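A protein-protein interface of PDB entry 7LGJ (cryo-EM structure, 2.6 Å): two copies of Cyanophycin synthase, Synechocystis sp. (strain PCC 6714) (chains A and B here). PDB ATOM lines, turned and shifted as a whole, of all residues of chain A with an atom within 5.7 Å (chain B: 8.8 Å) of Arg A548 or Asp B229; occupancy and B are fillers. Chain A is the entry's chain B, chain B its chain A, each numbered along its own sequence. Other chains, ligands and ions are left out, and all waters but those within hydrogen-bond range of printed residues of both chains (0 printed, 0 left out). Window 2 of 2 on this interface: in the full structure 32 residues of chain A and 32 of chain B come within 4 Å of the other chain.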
ATOM      1  N   MET A 182      13.587  14.602  17.992  1.00  0.00           N
ATOM      2  CA  MET A 182      12.420  13.724  17.938  1.00  0.00           C
ATOM      3  C   MET A 182      12.288  12.949  16.649  1.00  0.00           C
ATOM      4  O   MET A 182      12.583  13.467  15.578  1.00  0.00           O
ATOM      5  CB  MET A 182      11.189  14.610  18.029  1.00  0.00           C
ATOM      6  CG  MET A 182      10.987  15.339  19.330  1.00  0.00           C
ATOM      7  SD  MET A 182      10.200  16.924  19.099  1.00  0.00           S
ATOM      8  CE  MET A 182      11.717  17.860  18.670  1.00  0.00           C
ATOM      9  N   LEU A 184       9.797  11.646  13.752  1.00  0.00           N
ATOM     10  CA  LEU A 184       8.483  11.989  13.251  1.00  0.00           C
ATOM     11  C   LEU A 184       7.771  10.766  12.722  1.00  0.00           C
ATOM     12  O   LEU A 184       8.386   9.761  12.374  1.00  0.00           O
ATOM     13  CB  LEU A 184       8.583  13.082  12.189  1.00  0.00           C
ATOM     14  CG  LEU A 184       9.269  14.389  12.630  1.00  0.00           C
ATOM     15  CD1 LEU A 184       9.347  15.317  11.443  1.00  0.00           C
ATOM     16  CD2 LEU A 184       8.506  15.038  13.789  1.00  0.00           C
ATOM     17  N   SER A 185       6.457  10.871  12.641  1.00  0.00           N
ATOM     18  CA  SER A 185       5.557   9.816  12.195  1.00  0.00           C
ATOM     19  C   SER A 185       5.582   9.450  10.704  1.00  0.00           C
ATOM     20  O   SER A 185       4.961   8.463  10.311  1.00  0.00           O
ATOM     21  CB  SER A 185       4.164  10.173  12.661  1.00  0.00           C
ATOM     22  OG  SER A 185       3.713  11.359  12.084  1.00  0.00           O
ATOM     23  N   GLN A 191      13.171  15.492  13.655  1.00  0.00           N
ATOM     24  CA  GLN A 191      13.068  16.906  13.974  1.00  0.00           C
ATOM     25  C   GLN A 191      14.121  17.334  14.984  1.00  0.00           C
ATOM     26  O   GLN A 191      14.352  16.651  15.979  1.00  0.00           O
ATOM     27  CB  GLN A 191      11.691  17.266  14.500  1.00  0.00           C
ATOM     28  CG  GLN A 191      11.535  18.742  14.835  1.00  0.00           C
ATOM     29  CD  GLN A 191      10.203  19.104  15.325  1.00  0.00           C
ATOM     30  OE1 GLN A 191       9.195  18.588  14.850  1.00  0.00           O
ATOM     31  NE2 GLN A 191      10.166  20.003  16.301  1.00  0.00           N
ATOM     32  N   GLY A 195       9.383  24.475  18.312  1.00  0.00           N
ATOM     33  CA  GLY A 195       8.562  25.602  17.848  1.00  0.00           C
ATOM     34  C   GLY A 195       9.071  26.207  16.564  1.00  0.00           C
ATOM     35  O   GLY A 195       9.463  25.501  15.637  1.00  0.00           O
ATOM     36  N   GLN A 198      12.563  24.930  14.825  1.00  0.00           N
ATOM     37  CA  GLN A 198      12.748  23.576  14.371  1.00  0.00           C
ATOM     38  C   GLN A 198      13.324  23.451  12.961  1.00  0.00           C
ATOM     39  O   GLN A 198      13.016  24.242  12.070  1.00  0.00           O
ATOM     40  CB  GLN A 198      11.432  22.821  14.421  1.00  0.00           C
ATOM     41  CG  GLN A 198      10.405  23.245  13.395  1.00  0.00           C
ATOM     42  CD  GLN A 198       9.173  22.438  13.493  1.00  0.00           C
ATOM     43  OE1 GLN A 198       9.052  21.416  12.820  1.00  0.00           O
ATOM     44  NE2 GLN A 198       8.265  22.847  14.334  1.00  0.00           N
ATOM     45  N   ARG A 200      14.345  20.008  10.056  1.00  0.00           N
ATOM     46  CA  ARG A 200      14.168  18.581   9.794  1.00  0.00           C
ATOM     47  C   ARG A 200      15.307  18.030   8.977  1.00  0.00           C
ATOM     48  O   ARG A 200      15.863  18.716   8.110  1.00  0.00           O
ATOM     49  CB  ARG A 200      12.876  18.294   9.043  1.00  0.00           C
ATOM     50  CG  ARG A 200      11.625  18.589   9.791  1.00  0.00           C
ATOM     51  CD  ARG A 200      10.408  18.348   8.988  1.00  0.00           C
ATOM     52  NE  ARG A 200       9.227  18.737   9.741  1.00  0.00           N
ATOM     53  CZ  ARG A 200       7.990  18.982   9.246  1.00  0.00           C
ATOM     54  NH1 ARG A 200       7.697  18.889   7.981  1.00  0.00           N
ATOM     55  NH2 ARG A 200       7.027  19.358  10.052  1.00  0.00           N
ATOM     56  N   GLU A 533      -7.598  21.679  19.739  1.00  0.00           N
ATOM     57  CA  GLU A 533      -8.274  20.452  20.193  1.00  0.00           C
ATOM     58  C   GLU A 533      -9.057  20.720  21.467  1.00  0.00           C
ATOM     59  O   GLU A 533      -8.653  21.554  22.266  1.00  0.00           O
ATOM     60  CB  GLU A 533      -7.305  19.281  20.445  1.00  0.00           C
ATOM     61  CG  GLU A 533      -6.529  18.825  19.223  1.00  0.00           C
ATOM     62  CD  GLU A 533      -5.699  17.580  19.389  1.00  0.00           C
ATOM     63  OE1 GLU A 533      -5.748  16.979  20.426  1.00  0.00           O
ATOM     64  OE2 GLU A 533      -5.014  17.234  18.454  1.00  0.00           O
ATOM     65  N   GLN A 541       1.441  13.836  25.511  1.00  0.00           N
ATOM     66  CA  GLN A 541       1.026  13.740  24.136  1.00  0.00           C
ATOM     67  C   GLN A 541       0.538  15.076  23.622  1.00  0.00           C
ATOM     68  O   GLN A 541       0.608  15.342  22.426  1.00  0.00           O
ATOM     69  CB  GLN A 541      -0.056  12.688  23.974  1.00  0.00           C
ATOM     70  CG  GLN A 541       0.427  11.260  24.143  1.00  0.00           C
ATOM     71  CD  GLN A 541       0.679  10.857  25.600  1.00  0.00           C
ATOM     72  OE1 GLN A 541       0.026  11.357  26.540  1.00  0.00           O
ATOM     73  NE2 GLN A 541       1.644   9.955  25.779  1.00  0.00           N
ATOM     74  N   ALA A 543       1.573  18.049  25.019  1.00  0.00           N
ATOM     75  CA  ALA A 543       2.705  18.947  25.096  1.00  0.00           C
ATOM     76  C   ALA A 543       3.466  18.895  23.784  1.00  0.00           C
ATOM     77  O   ALA A 543       3.948  19.918  23.296  1.00  0.00           O
ATOM     78  CB  ALA A 543       3.596  18.574  26.249  1.00  0.00           C
ATOM     79  N   GLY A 544       3.506  17.705  23.178  1.00  0.00           N
ATOM     80  CA  GLY A 544       4.163  17.481  21.906  1.00  0.00           C
ATOM     81  C   GLY A 544       3.475  18.153  20.716  1.00  0.00           C
ATOM     82  O   GLY A 544       4.103  18.343  19.682  1.00  0.00           O
ATOM     83  N   VAL A 545       2.206  18.519  20.839  1.00  0.00           N
ATOM     84  CA  VAL A 545       1.499  19.174  19.757  1.00  0.00           C
ATOM     85  C   VAL A 545       2.001  20.592  19.702  1.00  0.00           C
ATOM     86  O   VAL A 545       2.276  21.116  18.629  1.00  0.00           O
ATOM     87  CB  VAL A 545      -0.031  19.131  19.954  1.00  0.00           C
ATOM     88  CG1 VAL A 545      -0.762  19.970  18.896  1.00  0.00           C
ATOM     89  CG2 VAL A 545      -0.483  17.716  19.871  1.00  0.00           C
ATOM     90  N   ILE A 546       2.119  21.216  20.870  1.00  0.00           N
ATOM     91  CA  ILE A 546       2.632  22.576  20.935  1.00  0.00           C
ATOM     92  C   ILE A 546       4.114  22.650  20.569  1.00  0.00           C
ATOM     93  O   ILE A 546       4.511  23.497  19.778  1.00  0.00           O
ATOM     94  CB  ILE A 546       2.398  23.203  22.340  1.00  0.00           C
ATOM     95  CG1 ILE A 546       0.883  23.359  22.657  1.00  0.00           C
ATOM     96  CG2 ILE A 546       3.117  24.550  22.492  1.00  0.00           C
ATOM     97  CD1 ILE A 546       0.084  24.252  21.701  1.00  0.00           C
ATOM     98  N   LEU A 547       4.938  21.748  21.084  1.00  0.00           N
ATOM     99  CA  LEU A 547       6.367  21.818  20.807  1.00  0.00           C
ATOM    100  C   LEU A 547       6.733  21.545  19.351  1.00  0.00           C
ATOM    101  O   LEU A 547       7.683  22.128  18.825  1.00  0.00           O
ATOM    102  CB  LEU A 547       7.117  20.890  21.762  1.00  0.00           C
ATOM    103  CG  LEU A 547       7.093  21.305  23.280  1.00  0.00           C
ATOM    104  CD1 LEU A 547       7.732  20.222  24.098  1.00  0.00           C
ATOM    105  CD2 LEU A 547       7.814  22.620  23.510  1.00  0.00           C
ATOM    106  N   ARG A 548       5.959  20.726  18.652  1.00  0.00           N
ATOM    107  CA  ARG A 548       6.236  20.471  17.247  1.00  0.00           C
ATOM    108  C   ARG A 548       5.633  21.518  16.303  1.00  0.00           C
ATOM    109  O   ARG A 548       5.835  21.436  15.094  1.00  0.00           O
ATOM    110  CB  ARG A 548       5.706  19.123  16.808  1.00  0.00           C
ATOM    111  CG  ARG A 548       6.393  17.901  17.369  1.00  0.00           C
ATOM    112  CD  ARG A 548       5.961  16.693  16.643  1.00  0.00           C
ATOM    113  NE  ARG A 548       4.523  16.451  16.764  1.00  0.00           N
ATOM    114  CZ  ARG A 548       3.908  15.722  17.718  1.00  0.00           C
ATOM    115  NH1 ARG A 548       4.601  15.120  18.658  1.00  0.00           N
ATOM    116  NH2 ARG A 548       2.587  15.615  17.705  1.00  0.00           N
ATOM    117  N   ASP A 549       4.849  22.464  16.817  1.00  0.00           N
ATOM    118  CA  ASP A 549       4.158  23.440  15.994  1.00  0.00           C
ATOM    119  C   ASP A 549       5.096  24.553  15.517  1.00  0.00           C
ATOM    120  O   ASP A 549       5.644  25.273  16.347  1.00  0.00           O
ATOM    121  CB  ASP A 549       2.955  24.017  16.720  1.00  0.00           C
ATOM    122  CG  ASP A 549       2.126  24.936  15.832  1.00  0.00           C
ATOM    123  OD1 ASP A 549       2.686  25.835  15.221  1.00  0.00           O
ATOM    124  OD2 ASP A 549       0.958  24.706  15.705  1.00  0.00           O
ATOM    125  N   PRO A 550       5.295  24.739  14.193  1.00  0.00           N
ATOM    126  CA  PRO A 550       6.235  25.648  13.557  1.00  0.00           C
ATOM    127  C   PRO A 550       5.976  27.124  13.790  1.00  0.00           C
ATOM    128  O   PRO A 550       6.790  27.948  13.389  1.00  0.00           O
ATOM    129  CB  PRO A 550       6.081  25.294  12.077  1.00  0.00           C
ATOM    130  CG  PRO A 550       4.714  24.743  11.942  1.00  0.00           C
ATOM    131  CD  PRO A 550       4.458  24.007  13.199  1.00  0.00           C
ATOM    132  N   GLU B 221      -0.555   9.233   2.063  1.00  0.00           N
ATOM    133  CA  GLU B 221      -0.646   8.614   3.371  1.00  0.00           C
ATOM    134  C   GLU B 221       0.224   9.363   4.372  1.00  0.00           C
ATOM    135  O   GLU B 221      -0.169   9.551   5.537  1.00  0.00           O
ATOM    136  CB  GLU B 221      -0.262   7.142   3.256  1.00  0.00           C
ATOM    137  CG  GLU B 221      -1.293   6.295   2.463  1.00  0.00           C
ATOM    138  CD  GLU B 221      -1.240   6.510   0.970  1.00  0.00           C
ATOM    139  OE1 GLU B 221      -0.324   7.164   0.510  1.00  0.00           O
ATOM    140  OE2 GLU B 221      -2.088   5.983   0.276  1.00  0.00           O
ATOM    141  N   GLY B 222       1.408   9.781   3.926  1.00  0.00           N
ATOM    142  CA  GLY B 222       2.337  10.526   4.746  1.00  0.00           C
ATOM    143  C   GLY B 222       1.768  11.875   5.122  1.00  0.00           C
ATOM    144  O   GLY B 222       1.822  12.262   6.289  1.00  0.00           O
ATOM    145  N   THR B 223       1.175  12.570   4.155  1.00  0.00           N
ATOM    146  CA  THR B 223       0.611  13.888   4.380  1.00  0.00           C
ATOM    147  C   THR B 223      -0.510  13.818   5.383  1.00  0.00           C
ATOM    148  O   THR B 223      -0.543  14.610   6.322  1.00  0.00           O
ATOM    149  CB  THR B 223       0.068  14.486   3.063  1.00  0.00           C
ATOM    150  OG1 THR B 223       1.116  14.639   2.138  1.00  0.00           O
ATOM    151  CG2 THR B 223      -0.556  15.849   3.280  1.00  0.00           C
ATOM    152  N   LYS B 224      -1.408  12.848   5.226  1.00  0.00           N
ATOM    153  CA  LYS B 224      -2.527  12.705   6.130  1.00  0.00           C
ATOM    154  C   LYS B 224      -2.073  12.434   7.550  1.00  0.00           C
ATOM    155  O   LYS B 224      -2.624  13.008   8.489  1.00  0.00           O
ATOM    156  CB  LYS B 224      -3.439  11.603   5.650  1.00  0.00           C
ATOM    157  CG  LYS B 224      -4.662  11.423   6.478  1.00  0.00           C
ATOM    158  CD  LYS B 224      -5.556  10.378   5.887  1.00  0.00           C
ATOM    159  CE  LYS B 224      -6.884  10.288   6.612  1.00  0.00           C
ATOM    160  NZ  LYS B 224      -6.798   9.686   7.999  1.00  0.00           N
ATOM    161  N   THR B 225      -1.070  11.575   7.715  1.00  0.00           N
ATOM    162  CA  THR B 225      -0.552  11.235   9.025  1.00  0.00           C
ATOM    163  C   THR B 225       0.010  12.469   9.726  1.00  0.00           C
ATOM    164  O   THR B 225      -0.342  12.754  10.870  1.00  0.00           O
ATOM    165  CB  THR B 225       0.555  10.171   8.868  1.00  0.00           C
ATOM    166  OG1 THR B 225      -0.001   8.988   8.283  1.00  0.00           O
ATOM    167  CG2 THR B 225       1.169   9.830  10.191  1.00  0.00           C
ATOM    168  N   ILE B 226       0.813  13.250   9.012  1.00  0.00           N
ATOM    169  CA  ILE B 226       1.413  14.445   9.575  1.00  0.00           C
ATOM    170  C   ILE B 226       0.373  15.482   9.945  1.00  0.00           C
ATOM    171  O   ILE B 226       0.508  16.139  10.974  1.00  0.00           O
ATOM    172  CB  ILE B 226       2.469  15.043   8.603  1.00  0.00           C
ATOM    173  CG1 ILE B 226       3.699  14.093   8.433  1.00  0.00           C
ATOM    174  CG2 ILE B 226       2.904  16.430   9.010  1.00  0.00           C
ATOM    175  CD1 ILE B 226       4.542  13.808   9.680  1.00  0.00           C
ATOM    176  N   LEU B 227      -0.633  15.694   9.105  1.00  0.00           N
ATOM    177  CA  LEU B 227      -1.623  16.691   9.440  1.00  0.00           C
ATOM    178  C   LEU B 227      -2.558  16.280  10.564  1.00  0.00           C
ATOM    179  O   LEU B 227      -2.835  17.089  11.452  1.00  0.00           O
ATOM    180  CB  LEU B 227      -2.459  17.036   8.210  1.00  0.00           C
ATOM    181  CG  LEU B 227      -1.750  17.750   7.055  1.00  0.00           C
ATOM    182  CD1 LEU B 227      -2.713  17.884   5.926  1.00  0.00           C
ATOM    183  CD2 LEU B 227      -1.224  19.116   7.469  1.00  0.00           C
ATOM    184  N   GLN B 228      -2.980  15.023  10.644  1.00  0.00           N
ATOM    185  CA  GLN B 228      -3.900  14.717  11.731  1.00  0.00           C
ATOM    186  C   GLN B 228      -3.180  14.743  13.081  1.00  0.00           C
ATOM    187  O   GLN B 228      -3.778  15.096  14.097  1.00  0.00           O
ATOM    188  CB  GLN B 228      -4.654  13.417  11.470  1.00  0.00           C
ATOM    189  CG  GLN B 228      -3.881  12.173  11.553  1.00  0.00           C
ATOM    190  CD  GLN B 228      -4.673  10.991  11.009  1.00  0.00           C
ATOM    191  OE1 GLN B 228      -5.503  11.142  10.091  1.00  0.00           O
ATOM    192  NE2 GLN B 228      -4.428   9.818  11.569  1.00  0.00           N
ATOM    193  N   ASP B 229      -1.860  14.539  13.087  1.00  0.00           N
ATOM    194  CA  ASP B 229      -1.061  14.616  14.308  1.00  0.00           C
ATOM    195  C   ASP B 229      -0.902  16.055  14.810  1.00  0.00           C
ATOM    196  O   ASP B 229      -0.397  16.281  15.911  1.00  0.00           O
ATOM    197  CB  ASP B 229       0.345  14.031  14.118  1.00  0.00           C
ATOM    198  CG  ASP B 229       0.431  12.492  14.025  1.00  0.00           C
ATOM    199  OD1 ASP B 229      -0.523  11.823  14.358  1.00  0.00           O
ATOM    200  OD2 ASP B 229       1.490  11.994  13.661  1.00  0.00           O
ATOM    201  N   ALA B 230      -1.251  17.036  13.972  1.00  0.00           N
ATOM    202  CA  ALA B 230      -1.156  18.451  14.267  1.00  0.00           C
ATOM    203  C   ALA B 230      -2.516  19.036  14.630  1.00  0.00           C
ATOM    204  O   ALA B 230      -2.641  20.257  14.805  1.00  0.00           O
ATOM    205  CB  ALA B 230      -0.594  19.179  13.063  1.00  0.00           C
ATOM    206  N   GLY B 231      -3.552  18.194  14.687  1.00  0.00           N
ATOM    207  CA  GLY B 231      -4.893  18.672  14.975  1.00  0.00           C
ATOM    208  C   GLY B 231      -5.619  19.283  13.770  1.00  0.00           C
ATOM    209  O   GLY B 231      -6.507  20.114  13.942  1.00  0.00           O
ATOM    210  N   ILE B 232      -5.240  18.913  12.546  1.00  0.00           N
ATOM    211  CA  ILE B 232      -5.845  19.452  11.333  1.00  0.00           C
ATOM    212  C   ILE B 232      -6.895  18.471  10.763  1.00  0.00           C
ATOM    213  O   ILE B 232      -6.606  17.282  10.673  1.00  0.00           O
ATOM    214  CB  ILE B 232      -4.716  19.769  10.337  1.00  0.00           C
ATOM    215  CG1 ILE B 232      -3.818  20.874  10.990  1.00  0.00           C
ATOM    216  CG2 ILE B 232      -5.239  20.127   8.960  1.00  0.00           C
ATOM    217  CD1 ILE B 232      -2.517  21.164  10.333  1.00  0.00           C
ATOM    218  N   PRO B 233      -8.155  18.897  10.467  1.00  0.00           N
ATOM    219  CA  PRO B 233      -9.226  18.042   9.946  1.00  0.00           C
ATOM    220  C   PRO B 233      -8.981  17.498   8.539  1.00  0.00           C
ATOM    221  O   PRO B 233      -8.808  18.263   7.591  1.00  0.00           O
ATOM    222  CB  PRO B 233     -10.424  18.991   9.945  1.00  0.00           C
ATOM    223  CG  PRO B 233      -9.839  20.372   9.873  1.00  0.00           C
ATOM    224  CD  PRO B 233      -8.538  20.301  10.627  1.00  0.00           C
ATOM    225  N   VAL B 234      -9.029  16.182   8.425  1.00  0.00           N
ATOM    226  CA  VAL B 234      -8.809  15.444   7.192  1.00  0.00           C
ATOM    227  C   VAL B 234      -9.906  14.382   7.098  1.00  0.00           C
ATOM    228  O   VAL B 234     -10.523  14.107   8.119  1.00  0.00           O
ATOM    229  CB  VAL B 234      -7.381  14.835   7.178  1.00  0.00           C
ATOM    230  CG1 VAL B 234      -6.308  15.943   7.221  1.00  0.00           C
ATOM    231  CG2 VAL B 234      -7.212  13.921   8.356  1.00  0.00           C
ATOM    232  N   ARG B 418      -1.219  27.525   8.519  1.00  0.00           N
ATOM    233  CA  ARG B 418      -0.612  26.537   9.398  1.00  0.00           C
ATOM    234  C   ARG B 418      -0.360  25.228   8.638  1.00  0.00           C
ATOM    235  O   ARG B 418       0.681  24.613   8.834  1.00  0.00           O
ATOM    236  CB  ARG B 418      -1.457  26.317  10.659  1.00  0.00           C
ATOM    237  CG  ARG B 418      -0.727  25.570  11.798  1.00  0.00           C
ATOM    238  CD  ARG B 418      -1.395  25.717  13.154  1.00  0.00           C
ATOM    239  NE  ARG B 418      -2.598  24.920  13.353  1.00  0.00           N
ATOM    240  CZ  ARG B 418      -2.616  23.631  13.815  1.00  0.00           C
ATOM    241  NH1 ARG B 418      -1.521  22.997  14.129  1.00  0.00           N
ATOM    242  NH2 ARG B 418      -3.743  22.973  13.971  1.00  0.00           N
ATOM    243  N   LYS B 421       2.850  25.384   6.502  1.00  0.00           N
ATOM    244  CA  LYS B 421       4.022  25.377   7.374  1.00  0.00           C
ATOM    245  C   LYS B 421       4.323  23.999   7.957  1.00  0.00           C
ATOM    246  O   LYS B 421       5.484  23.615   8.039  1.00  0.00           O
ATOM    247  CB  LYS B 421       3.842  26.414   8.461  1.00  0.00           C
ATOM    248  CG  LYS B 421       3.905  27.823   7.930  1.00  0.00           C
ATOM    249  CD  LYS B 421       3.622  28.849   8.992  1.00  0.00           C
ATOM    250  CE  LYS B 421       3.562  30.244   8.390  1.00  0.00           C
ATOM    251  NZ  LYS B 421       3.182  31.276   9.381  1.00  0.00           N
ATOM    252  N   VAL B 422       3.285  23.239   8.310  1.00  0.00           N
ATOM    253  CA  VAL B 422       3.422  21.883   8.834  1.00  0.00           C
ATOM    254  C   VAL B 422       4.022  20.944   7.790  1.00  0.00           C
ATOM    255  O   VAL B 422       4.878  20.114   8.127  1.00  0.00           O
ATOM    256  CB  VAL B 422       2.055  21.355   9.340  1.00  0.00           C
ATOM    257  CG1 VAL B 422       2.109  19.894   9.668  1.00  0.00           C
ATOM    258  CG2 VAL B 422       1.667  22.093  10.607  1.00  0.00           C
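OG of Ser A185 lies within hydrogen-bond range of OD2 of Asp B229, 2.8 Å away. The guanidinium group (NH1) of Arg B418 is in salt-bridge range of the side-chain carboxylate (OD2) of Asp A549, 3.4 Å away. The backbone carbonyl oxygen (O) of Val B422 lies within hydrogen-bond range of the guanidinium group (NH2) of Arg A200, at 3.0 Å.
OG1 of Thr B225 sits at hydrogen-bond distance from O of Glu B221. The guanidinium group of Arg B418 lies within hydrogen-bond range of the backbone carbonyl oxygen of Ala B230 (3.0 Å). The side-chain amide nitrogen (NE2) of Gln A198 is in hydrogen-bond range of the backbone carbonyl oxygen (O) of Arg A548. The backbone carbonyl oxygen (O) of Gly A544 lies close to the guanidinium group (NH1) of Arg A548 (3.4 Å).
CG2 of Thr B225 touches OG of Ser A185, at 3.5 Å. CD1 of Ile B226 touches OG of Ser A185, 3.5 Å away. Gly B231 touches Glu A533. O of Asp B229 touches NH2 of Arg A548, 3.5 Å away. Pro A550 touches Lys B421 (CG to CB, 3.96 Å).
Arg A548 touches just one residue of chain B: Asp B229 (3.5 Å). Asp B229 touches just these residues of chain A: Ser A185 (2.8 Å) and Arg A548 (3.5 Å). Of the printed residues of chain B, Glu A533 touches Gly B231 (3.8 Å). Printed residues of chain A within 4 Å of Thr B225: Ser A185. The nearest residue of chain B that does not touch Arg A548 is Ala B230 (5.5 Å). The nearest printed residue of chain A that does not touch Gly B231 is Val A545 (5.4 Å).
Hydrophobic or aromatic side chains of chain A that line the printed part of chain B: Pro A550. Of the 17 printed residues of chain B, 7 touch a printed residue of chain A. Printed residues of chain B that touch a printed residue of chain A: Thr B225, Ile B226, Asp B229, Gly B231, Arg B418, Lys B421 and Val B422. Hydrophobic or aromatic side chains of chain B that line the printed part of chain A: Ile B226. Along chain B the printed residues that touch a printed residue of chain A span positions 225 to 422. Among the printed residues, 8 pairs touch across the chains.
No position is printed for both chains. Of the 8 pairs that touch across the chains among the printed residues, none has its exchanged pair printed and touching as well.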
